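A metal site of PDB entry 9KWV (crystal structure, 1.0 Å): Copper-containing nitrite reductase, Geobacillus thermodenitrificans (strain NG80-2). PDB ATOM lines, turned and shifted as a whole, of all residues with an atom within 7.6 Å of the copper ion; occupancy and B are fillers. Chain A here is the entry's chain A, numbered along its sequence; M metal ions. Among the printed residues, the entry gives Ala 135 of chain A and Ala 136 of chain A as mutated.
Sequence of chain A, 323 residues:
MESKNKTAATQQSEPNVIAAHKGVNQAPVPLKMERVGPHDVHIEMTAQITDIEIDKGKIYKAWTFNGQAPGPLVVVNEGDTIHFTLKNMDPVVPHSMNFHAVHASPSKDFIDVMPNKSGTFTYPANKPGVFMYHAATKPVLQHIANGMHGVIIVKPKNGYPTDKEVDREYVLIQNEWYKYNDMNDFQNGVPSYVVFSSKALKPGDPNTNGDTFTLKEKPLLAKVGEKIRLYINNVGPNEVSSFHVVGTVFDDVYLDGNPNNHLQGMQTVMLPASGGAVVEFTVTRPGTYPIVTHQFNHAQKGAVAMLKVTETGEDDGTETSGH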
ATOM      1  N   ALA A  47      25.727  -2.958  20.673  1.00  0.00           N
ATOM      2  CA  ALA A  47      26.813  -3.194  19.723  1.00  0.00           C
ATOM      3  C   ALA A  47      27.864  -3.998  20.470  1.00  0.00           C
ATOM      4  O   ALA A  47      28.303  -3.589  21.556  1.00  0.00           O
ATOM      5  CB  ALA A  47      27.405  -1.876  19.220  1.00  0.00           C
ATOM      6  N   GLN A  48      28.244  -5.150  19.936  1.00  0.00           N
ATOM      7  CA  GLN A  48      29.134  -6.042  20.663  1.00  0.00           C
ATOM      8  C   GLN A  48      29.919  -6.918  19.694  1.00  0.00           C
ATOM      9  O   GLN A  48      29.535  -7.096  18.529  1.00  0.00           O
ATOM     10  CB  GLN A  48      28.345  -6.885  21.682  1.00  0.00           C
ATOM     11  CG  GLN A  48      27.306  -7.804  21.057  1.00  0.00           C
ATOM     12  CD  GLN A  48      26.570  -8.582  22.121  1.00  0.00           C
ATOM     13  OE1 GLN A  48      25.620  -8.096  22.737  1.00  0.00           O
ATOM     14  NE2 GLN A  48      27.033  -9.782  22.391  1.00  0.00           N
ATOM     15  N   ILE A  49      31.025  -7.441  20.197  1.00  0.00           N
ATOM     16  CA  ILE A  49      32.008  -8.197  19.429  1.00  0.00           C
ATOM     17  C   ILE A  49      31.854  -9.663  19.799  1.00  0.00           C
ATOM     18  O   ILE A  49      32.080 -10.032  20.963  1.00  0.00           O
ATOM     19  CB  ILE A  49      33.421  -7.681  19.742  1.00  0.00           C
ATOM     20  CG1 ILE A  49      33.551  -6.162  19.449  1.00  0.00           C
ATOM     21  CG2 ILE A  49      34.472  -8.495  18.991  1.00  0.00           C
ATOM     22  CD1 ILE A  49      33.183  -5.767  18.021  1.00  0.00           C
ATOM     23  N   TRP A  63      31.482  -7.844  14.214  1.00  0.00           N
ATOM     24  CA  TRP A  63      30.918  -6.629  14.781  1.00  0.00           C
ATOM     25  C   TRP A  63      29.414  -6.754  14.644  1.00  0.00           C
ATOM     26  O   TRP A  63      28.902  -6.843  13.532  1.00  0.00           O
ATOM     27  CB  TRP A  63      31.413  -5.410  14.018  1.00  0.00           C
ATOM     28  CG  TRP A  63      32.902  -5.154  14.022  1.00  0.00           C
ATOM     29  CD1 TRP A  63      33.906  -5.971  14.487  1.00  0.00           C
ATOM     30  CD2 TRP A  63      33.543  -3.990  13.508  1.00  0.00           C
ATOM     31  NE1 TRP A  63      35.126  -5.356  14.298  1.00  0.00           N
ATOM     32  CE2 TRP A  63      34.923  -4.140  13.701  1.00  0.00           C
ATOM     33  CE3 TRP A  63      33.074  -2.829  12.885  1.00  0.00           C
ATOM     34  CZ2 TRP A  63      35.844  -3.174  13.284  1.00  0.00           C
ATOM     35  CZ3 TRP A  63      33.981  -1.872  12.477  1.00  0.00           C
ATOM     36  CH2 TRP A  63      35.346  -2.042  12.685  1.00  0.00           C
ATOM     37  N   THR A  64      28.694  -6.812  15.776  1.00  0.00           N
ATOM     38  CA  THR A  64      27.303  -7.232  15.765  1.00  0.00           C
ATOM     39  C   THR A  64      26.407  -6.302  16.560  1.00  0.00           C
ATOM     40  O   THR A  64      26.844  -5.579  17.461  1.00  0.00           O
ATOM     41  CB  THR A  64      27.097  -8.635  16.365  1.00  0.00           C
ATOM     42  OG1 THR A  64      27.198  -8.603  17.794  1.00  0.00           O
ATOM     43  CG2 THR A  64      28.084  -9.646  15.800  1.00  0.00           C
ATOM     44  N   PHE A  65      25.123  -6.373  16.219  1.00  0.00           N
ATOM     45  CA  PHE A  65      24.050  -5.997  17.121  1.00  0.00           C
ATOM     46  C   PHE A  65      23.631  -7.235  17.909  1.00  0.00           C
ATOM     47  O   PHE A  65      23.225  -8.250  17.329  1.00  0.00           O
ATOM     48  CB  PHE A  65      22.882  -5.412  16.347  1.00  0.00           C
ATOM     49  CG  PHE A  65      23.222  -4.151  15.576  1.00  0.00           C
ATOM     50  CD1 PHE A  65      23.485  -2.968  16.249  1.00  0.00           C
ATOM     51  CD2 PHE A  65      23.318  -4.160  14.200  1.00  0.00           C
ATOM     52  CE1 PHE A  65      23.798  -1.809  15.560  1.00  0.00           C
ATOM     53  CE2 PHE A  65      23.624  -2.988  13.502  1.00  0.00           C
ATOM     54  CZ  PHE A  65      23.872  -1.824  14.181  1.00  0.00           C
ATOM     55  N   LEU A  86      20.923   2.394  21.641  1.00  0.00           N
ATOM     56  CA  LEU A  86      22.070   1.546  21.373  1.00  0.00           C
ATOM     57  C   LEU A  86      23.044   1.656  22.534  1.00  0.00           C
ATOM     58  O   LEU A  86      23.484   2.757  22.886  1.00  0.00           O
ATOM     59  CB  LEU A  86      22.785   1.966  20.076  1.00  0.00           C
ATOM     60  CG  LEU A  86      23.965   1.079  19.642  1.00  0.00           C
ATOM     61  CD1 LEU A  86      23.508  -0.340  19.288  1.00  0.00           C
ATOM     62  CD2 LEU A  86      24.685   1.703  18.470  1.00  0.00           C
ATOM     63  N   ASN A  88      26.704   0.606  23.487  1.00  0.00           N
ATOM     64  CA  ASN A  88      27.935   0.176  22.816  1.00  0.00           C
ATOM     65  C   ASN A  88      28.847  -0.531  23.809  1.00  0.00           C
ATOM     66  O   ASN A  88      29.441   0.103  24.682  1.00  0.00           O
ATOM     67  CB  ASN A  88      28.659   1.349  22.160  1.00  0.00           C
ATOM     68  CG  ASN A  88      29.815   0.895  21.304  1.00  0.00           C
ATOM     69  OD1 ASN A  88      30.087  -0.302  21.200  1.00  0.00           O
ATOM     70  ND2 ASN A  88      30.507   1.840  20.689  1.00  0.00           N
ATOM     71  N   ASP A  90      31.461  -2.385  22.699  1.00  0.00           N
ATOM     72  CA  ASP A  90      32.787  -2.495  22.099  1.00  0.00           C
ATOM     73  C   ASP A  90      33.747  -1.646  22.919  1.00  0.00           C
ATOM     74  O   ASP A  90      33.444  -0.488  23.218  1.00  0.00           O
ATOM     75  CB  ASP A  90      32.692  -1.977  20.657  1.00  0.00           C
ATOM     76  CG  ASP A  90      33.954  -2.218  19.826  1.00  0.00           C
ATOM     77  OD1 ASP A  90      35.069  -2.022  20.353  1.00  0.00           O
ATOM     78  OD2 ASP A  90      33.799  -2.529  18.621  1.00  0.00           O
ATOM     79  N   VAL A  93      35.741   0.742  19.438  1.00  0.00           N
ATOM     80  CA  VAL A  93      35.179   1.239  18.181  1.00  0.00           C
ATOM     81  C   VAL A  93      33.810   1.855  18.431  1.00  0.00           C
ATOM     82  O   VAL A  93      32.944   1.197  19.034  1.00  0.00           O
ATOM     83  CB  VAL A  93      35.093   0.135  17.100  1.00  0.00           C
ATOM     84  CG1 VAL A  93      34.662   0.742  15.771  1.00  0.00           C
ATOM     85  CG2 VAL A  93      36.412  -0.593  16.949  1.00  0.00           C
ATOM     86  N   PRO A  94      33.551   3.083  17.951  1.00  0.00           N
ATOM     87  CA  PRO A  94      32.178   3.617  17.974  1.00  0.00           C
ATOM     88  C   PRO A  94      31.284   2.843  17.009  1.00  0.00           C
ATOM     89  O   PRO A  94      31.742   2.334  15.985  1.00  0.00           O
ATOM     90  CB  PRO A  94      32.355   5.065  17.501  1.00  0.00           C
ATOM     91  CG  PRO A  94      33.803   5.370  17.682  1.00  0.00           C
ATOM     92  CD  PRO A  94      34.494   4.068  17.398  1.00  0.00           C
ATOM     93  N   HIS A  95      29.994   2.800  17.324  1.00  0.00           N
ATOM     94  CA  HIS A  95      28.991   2.210  16.439  1.00  0.00           C
ATOM     95  C   HIS A  95      27.745   3.085  16.437  1.00  0.00           C
ATOM     96  O   HIS A  95      27.654   4.071  17.166  1.00  0.00           O
ATOM     97  CB  HIS A  95      28.674   0.752  16.835  1.00  0.00           C
ATOM     98  CG  HIS A  95      29.874  -0.145  16.839  1.00  0.00           C
ATOM     99  ND1 HIS A  95      30.468  -0.629  15.690  1.00  0.00           N
ATOM    100  CD2 HIS A  95      30.609  -0.616  17.873  1.00  0.00           C
ATOM    101  CE1 HIS A  95      31.517  -1.370  16.030  1.00  0.00           C
ATOM    102  NE2 HIS A  95      31.628  -1.372  17.353  1.00  0.00           N
ATOM    103  N   SER A  96      26.774   2.752  15.586  1.00  0.00           N
ATOM    104  CA  SER A  96      25.605   3.590  15.362  1.00  0.00           C
ATOM    105  C   SER A  96      24.555   2.739  14.655  1.00  0.00           C
ATOM    106  O   SER A  96      24.796   1.568  14.328  1.00  0.00           O
ATOM    107  CB  SER A  96      25.960   4.794  14.491  1.00  0.00           C
ATOM    108  OG  SER A  96      26.417   4.351  13.214  1.00  0.00           O
ATOM    109  N   HIS A 134      21.437  -1.104   9.602  1.00  0.00           N
ATOM    110  CA  HIS A 134      22.883  -1.330   9.626  1.00  0.00           C
ATOM    111  C   HIS A 134      23.547  -0.168  10.366  1.00  0.00           C
ATOM    112  O   HIS A 134      22.952   0.891  10.569  1.00  0.00           O
ATOM    113  CB  HIS A 134      23.458  -1.460   8.206  1.00  0.00           C
ATOM    114  CG  HIS A 134      23.216  -0.261   7.347  1.00  0.00           C
ATOM    115  ND1 HIS A 134      24.047   0.843   7.361  1.00  0.00           N
ATOM    116  CD2 HIS A 134      22.268   0.008   6.412  1.00  0.00           C
ATOM    117  CE1 HIS A 134      23.608   1.734   6.474  1.00  0.00           C
ATOM    118  NE2 HIS A 134      22.546   1.240   5.874  1.00  0.00           N
ATOM    119  N   ALA A 135      24.814  -0.366  10.722  1.00  0.00           N
ATOM    120  CA  ALA A 135      25.555   0.732  11.327  1.00  0.00           C
ATOM    121  C   ALA A 135      25.855   1.829  10.311  1.00  0.00           C
ATOM    122  O   ALA A 135      26.029   1.573   9.117  1.00  0.00           O
ATOM    123  CB  ALA A 135      26.849   0.220  11.962  1.00  0.00           C
ATOM    124  N   ALA A 136      25.946   3.068  10.804  1.00  0.00           N
ATOM    125  CA  ALA A 136      26.141   4.256   9.976  1.00  0.00           C
ATOM    126  C   ALA A 136      27.505   4.888  10.160  1.00  0.00           C
ATOM    127  O   ALA A 136      27.780   5.952   9.585  1.00  0.00           O
ATOM    128  CB  ALA A 136      25.023   5.278  10.224  1.00  0.00           C
ATOM    129  N   THR A 137      28.396   4.236  10.875  1.00  0.00           N
ATOM    130  CA  THR A 137      29.680   4.796  11.264  1.00  0.00           C
ATOM    131  C   THR A 137      30.673   4.644  10.126  1.00  0.00           C
ATOM    132  O   THR A 137      30.806   3.563   9.538  1.00  0.00           O
ATOM    133  CB  THR A 137      30.158   4.049  12.513  1.00  0.00           C
ATOM    134  OG1 THR A 137      29.186   4.180  13.569  1.00  0.00           O
ATOM    135  CG2 THR A 137      31.514   4.545  13.001  1.00  0.00           C
ATOM    136  N   PRO A 139      34.082   3.973   8.225  1.00  0.00           N
ATOM    137  CA  PRO A 139      33.549   3.627   6.896  1.00  0.00           C
ATOM    138  C   PRO A 139      32.397   2.646   7.023  1.00  0.00           C
ATOM    139  O   PRO A 139      32.549   1.573   7.629  1.00  0.00           O
ATOM    140  CB  PRO A 139      34.740   2.952   6.192  1.00  0.00           C
ATOM    141  CG  PRO A 139      35.886   3.028   7.121  1.00  0.00           C
ATOM    142  CD  PRO A 139      35.337   3.264   8.499  1.00  0.00           C
ATOM    143  N   VAL A 140      31.249   2.996   6.438  1.00  0.00           N
ATOM    144  CA  VAL A 140      30.077   2.154   6.564  1.00  0.00           C
ATOM    145  C   VAL A 140      30.337   0.764   5.990  1.00  0.00           C
ATOM    146  O   VAL A 140      29.889  -0.250   6.547  1.00  0.00           O
ATOM    147  CB  VAL A 140      28.850   2.847   5.945  1.00  0.00           C
ATOM    148  CG1 VAL A 140      27.673   1.913   5.843  1.00  0.00           C
ATOM    149  CG2 VAL A 140      28.477   4.076   6.788  1.00  0.00           C
ATOM    150  N   GLN A 142      32.975  -0.982   6.151  1.00  0.00           N
ATOM    151  CA  GLN A 142      33.670  -1.792   7.158  1.00  0.00           C
ATOM    152  C   GLN A 142      32.695  -2.351   8.194  1.00  0.00           C
ATOM    153  O   GLN A 142      32.777  -3.526   8.583  1.00  0.00           O
ATOM    154  CB  GLN A 142      34.742  -0.941   7.837  1.00  0.00           C
ATOM    155  CG  GLN A 142      35.660  -1.739   8.755  1.00  0.00           C
ATOM    156  CD  GLN A 142      36.797  -0.917   9.293  1.00  0.00           C
ATOM    157  OE1 GLN A 142      36.787   0.308   9.235  1.00  0.00           O
ATOM    158  NE2 GLN A 142      37.796  -1.591   9.832  1.00  0.00           N
ATOM    159  N   HIS A 143      31.771  -1.502   8.667  1.00  0.00           N
ATOM    160  CA  HIS A 143      30.813  -1.945   9.672  1.00  0.00           C
ATOM    161  C   HIS A 143      29.839  -2.973   9.117  1.00  0.00           C
ATOM    162  O   HIS A 143      29.551  -3.969   9.793  1.00  0.00           O
ATOM    163  CB  HIS A 143      30.067  -0.753  10.279  1.00  0.00           C
ATOM    164  CG  HIS A 143      30.927   0.081  11.179  1.00  0.00           C
ATOM    165  ND1 HIS A 143      30.848   0.025  12.556  1.00  0.00           N
ATOM    166  CD2 HIS A 143      31.939   0.934  10.885  1.00  0.00           C
ATOM    167  CE1 HIS A 143      31.759   0.837  13.060  1.00  0.00           C
ATOM    168  NE2 HIS A 143      32.435   1.397  12.066  1.00  0.00           N
ATOM    169  N   ILE A 144      29.318  -2.751   7.901  1.00  0.00           N
ATOM    170  CA  ILE A 144      28.415  -3.737   7.318  1.00  0.00           C
ATOM    171  C   ILE A 144      29.142  -5.054   7.076  1.00  0.00           C
ATOM    172  O   ILE A 144      28.682  -6.128   7.459  1.00  0.00           O
ATOM    173  CB  ILE A 144      27.749  -3.213   6.025  1.00  0.00           C
ATOM    174  CG1 ILE A 144      26.906  -1.951   6.297  1.00  0.00           C
ATOM    175  CG2 ILE A 144      26.877  -4.305   5.418  1.00  0.00           C
ATOM    176  CD1 ILE A 144      26.307  -1.344   5.044  1.00  0.00           C
ATOM    177  N   ASN A 146      31.700  -6.345   8.422  1.00  0.00           N
ATOM    178  CA  ASN A 146      32.054  -7.053   9.645  1.00  0.00           C
ATOM    179  C   ASN A 146      30.852  -7.608  10.405  1.00  0.00           C
ATOM    180  O   ASN A 146      31.055  -8.326  11.398  1.00  0.00           O
ATOM    181  CB  ASN A 146      32.893  -6.167  10.572  1.00  0.00           C
ATOM    182  CG  ASN A 146      34.353  -6.077  10.149  1.00  0.00           C
ATOM    183  OD1 ASN A 146      34.927  -7.005   9.588  1.00  0.00           O
ATOM    184  ND2 ASN A 146      34.976  -4.944  10.463  1.00  0.00           N
ATOM    185  N   GLY A 147      29.615  -7.341   9.971  1.00  0.00           N
ATOM    186  CA  GLY A 147      28.436  -7.989  10.525  1.00  0.00           C
ATOM    187  C   GLY A 147      27.301  -7.083  10.976  1.00  0.00           C
ATOM    188  O   GLY A 147      26.276  -7.618  11.421  1.00  0.00           O
ATOM    189  N   MET A 148      27.428  -5.756  10.886  1.00  0.00           N
ATOM    190  CA  MET A 148      26.447  -4.847  11.496  1.00  0.00           C
ATOM    191  C   MET A 148      25.363  -4.516  10.476  1.00  0.00           C
ATOM    192  O   MET A 148      25.277  -3.412   9.912  1.00  0.00           O
ATOM    193  CB  MET A 148      27.163  -3.604  12.010  1.00  0.00           C
ATOM    194  CG  MET A 148      27.888  -3.814  13.278  1.00  0.00           C
ATOM    195  SD  MET A 148      28.057  -2.299  14.281  1.00  0.00           S
ATOM    196  CE  MET A 148      28.279  -3.101  15.832  1.00  0.00           C
HETATM  197 CU    CU M   1      29.692  -0.988  13.786  1.00  0.00          CU
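OD2 of Asp 90 lies within hydrogen-bond range of NE2 of His 95, at 2.8 Å.
The backbone carbonyl oxygen (O) of Val 93 lies close to a ring nitrogen (NE2) of His 95, at 3.3 Å.
The backbone carbonyl oxygen (O) of Met 148 lies within hydrogen-bond range of the backbone NH (N) of Ala 135, at 3.2 Å.
N of Trp 63 is in hydrogen-bond range of O of Asn 146 (2.9 Å).
The backbone carbonyl oxygen of Trp 63 sits close to the backbone NH of Met 148, at 3.2 Å.
Trp 63 touches the copper ion (CE3 to CU, 3.95 Å).
CB of Ala 135 touches the copper ion, at 3.6 Å.
Five residues have an atom within 4 Å of the copper ion: Trp 63, His 95, Ala 135, His 143 and Met 148.
ND1 of His 143 is bound to the copper ion, at 2.0 Å.
ND1 of His 95 is bound to the copper ion (2.1 Å).
SD of Met 148 binds the copper ion (2.2 Å).
The copper ion has three donor atoms within binding distance.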
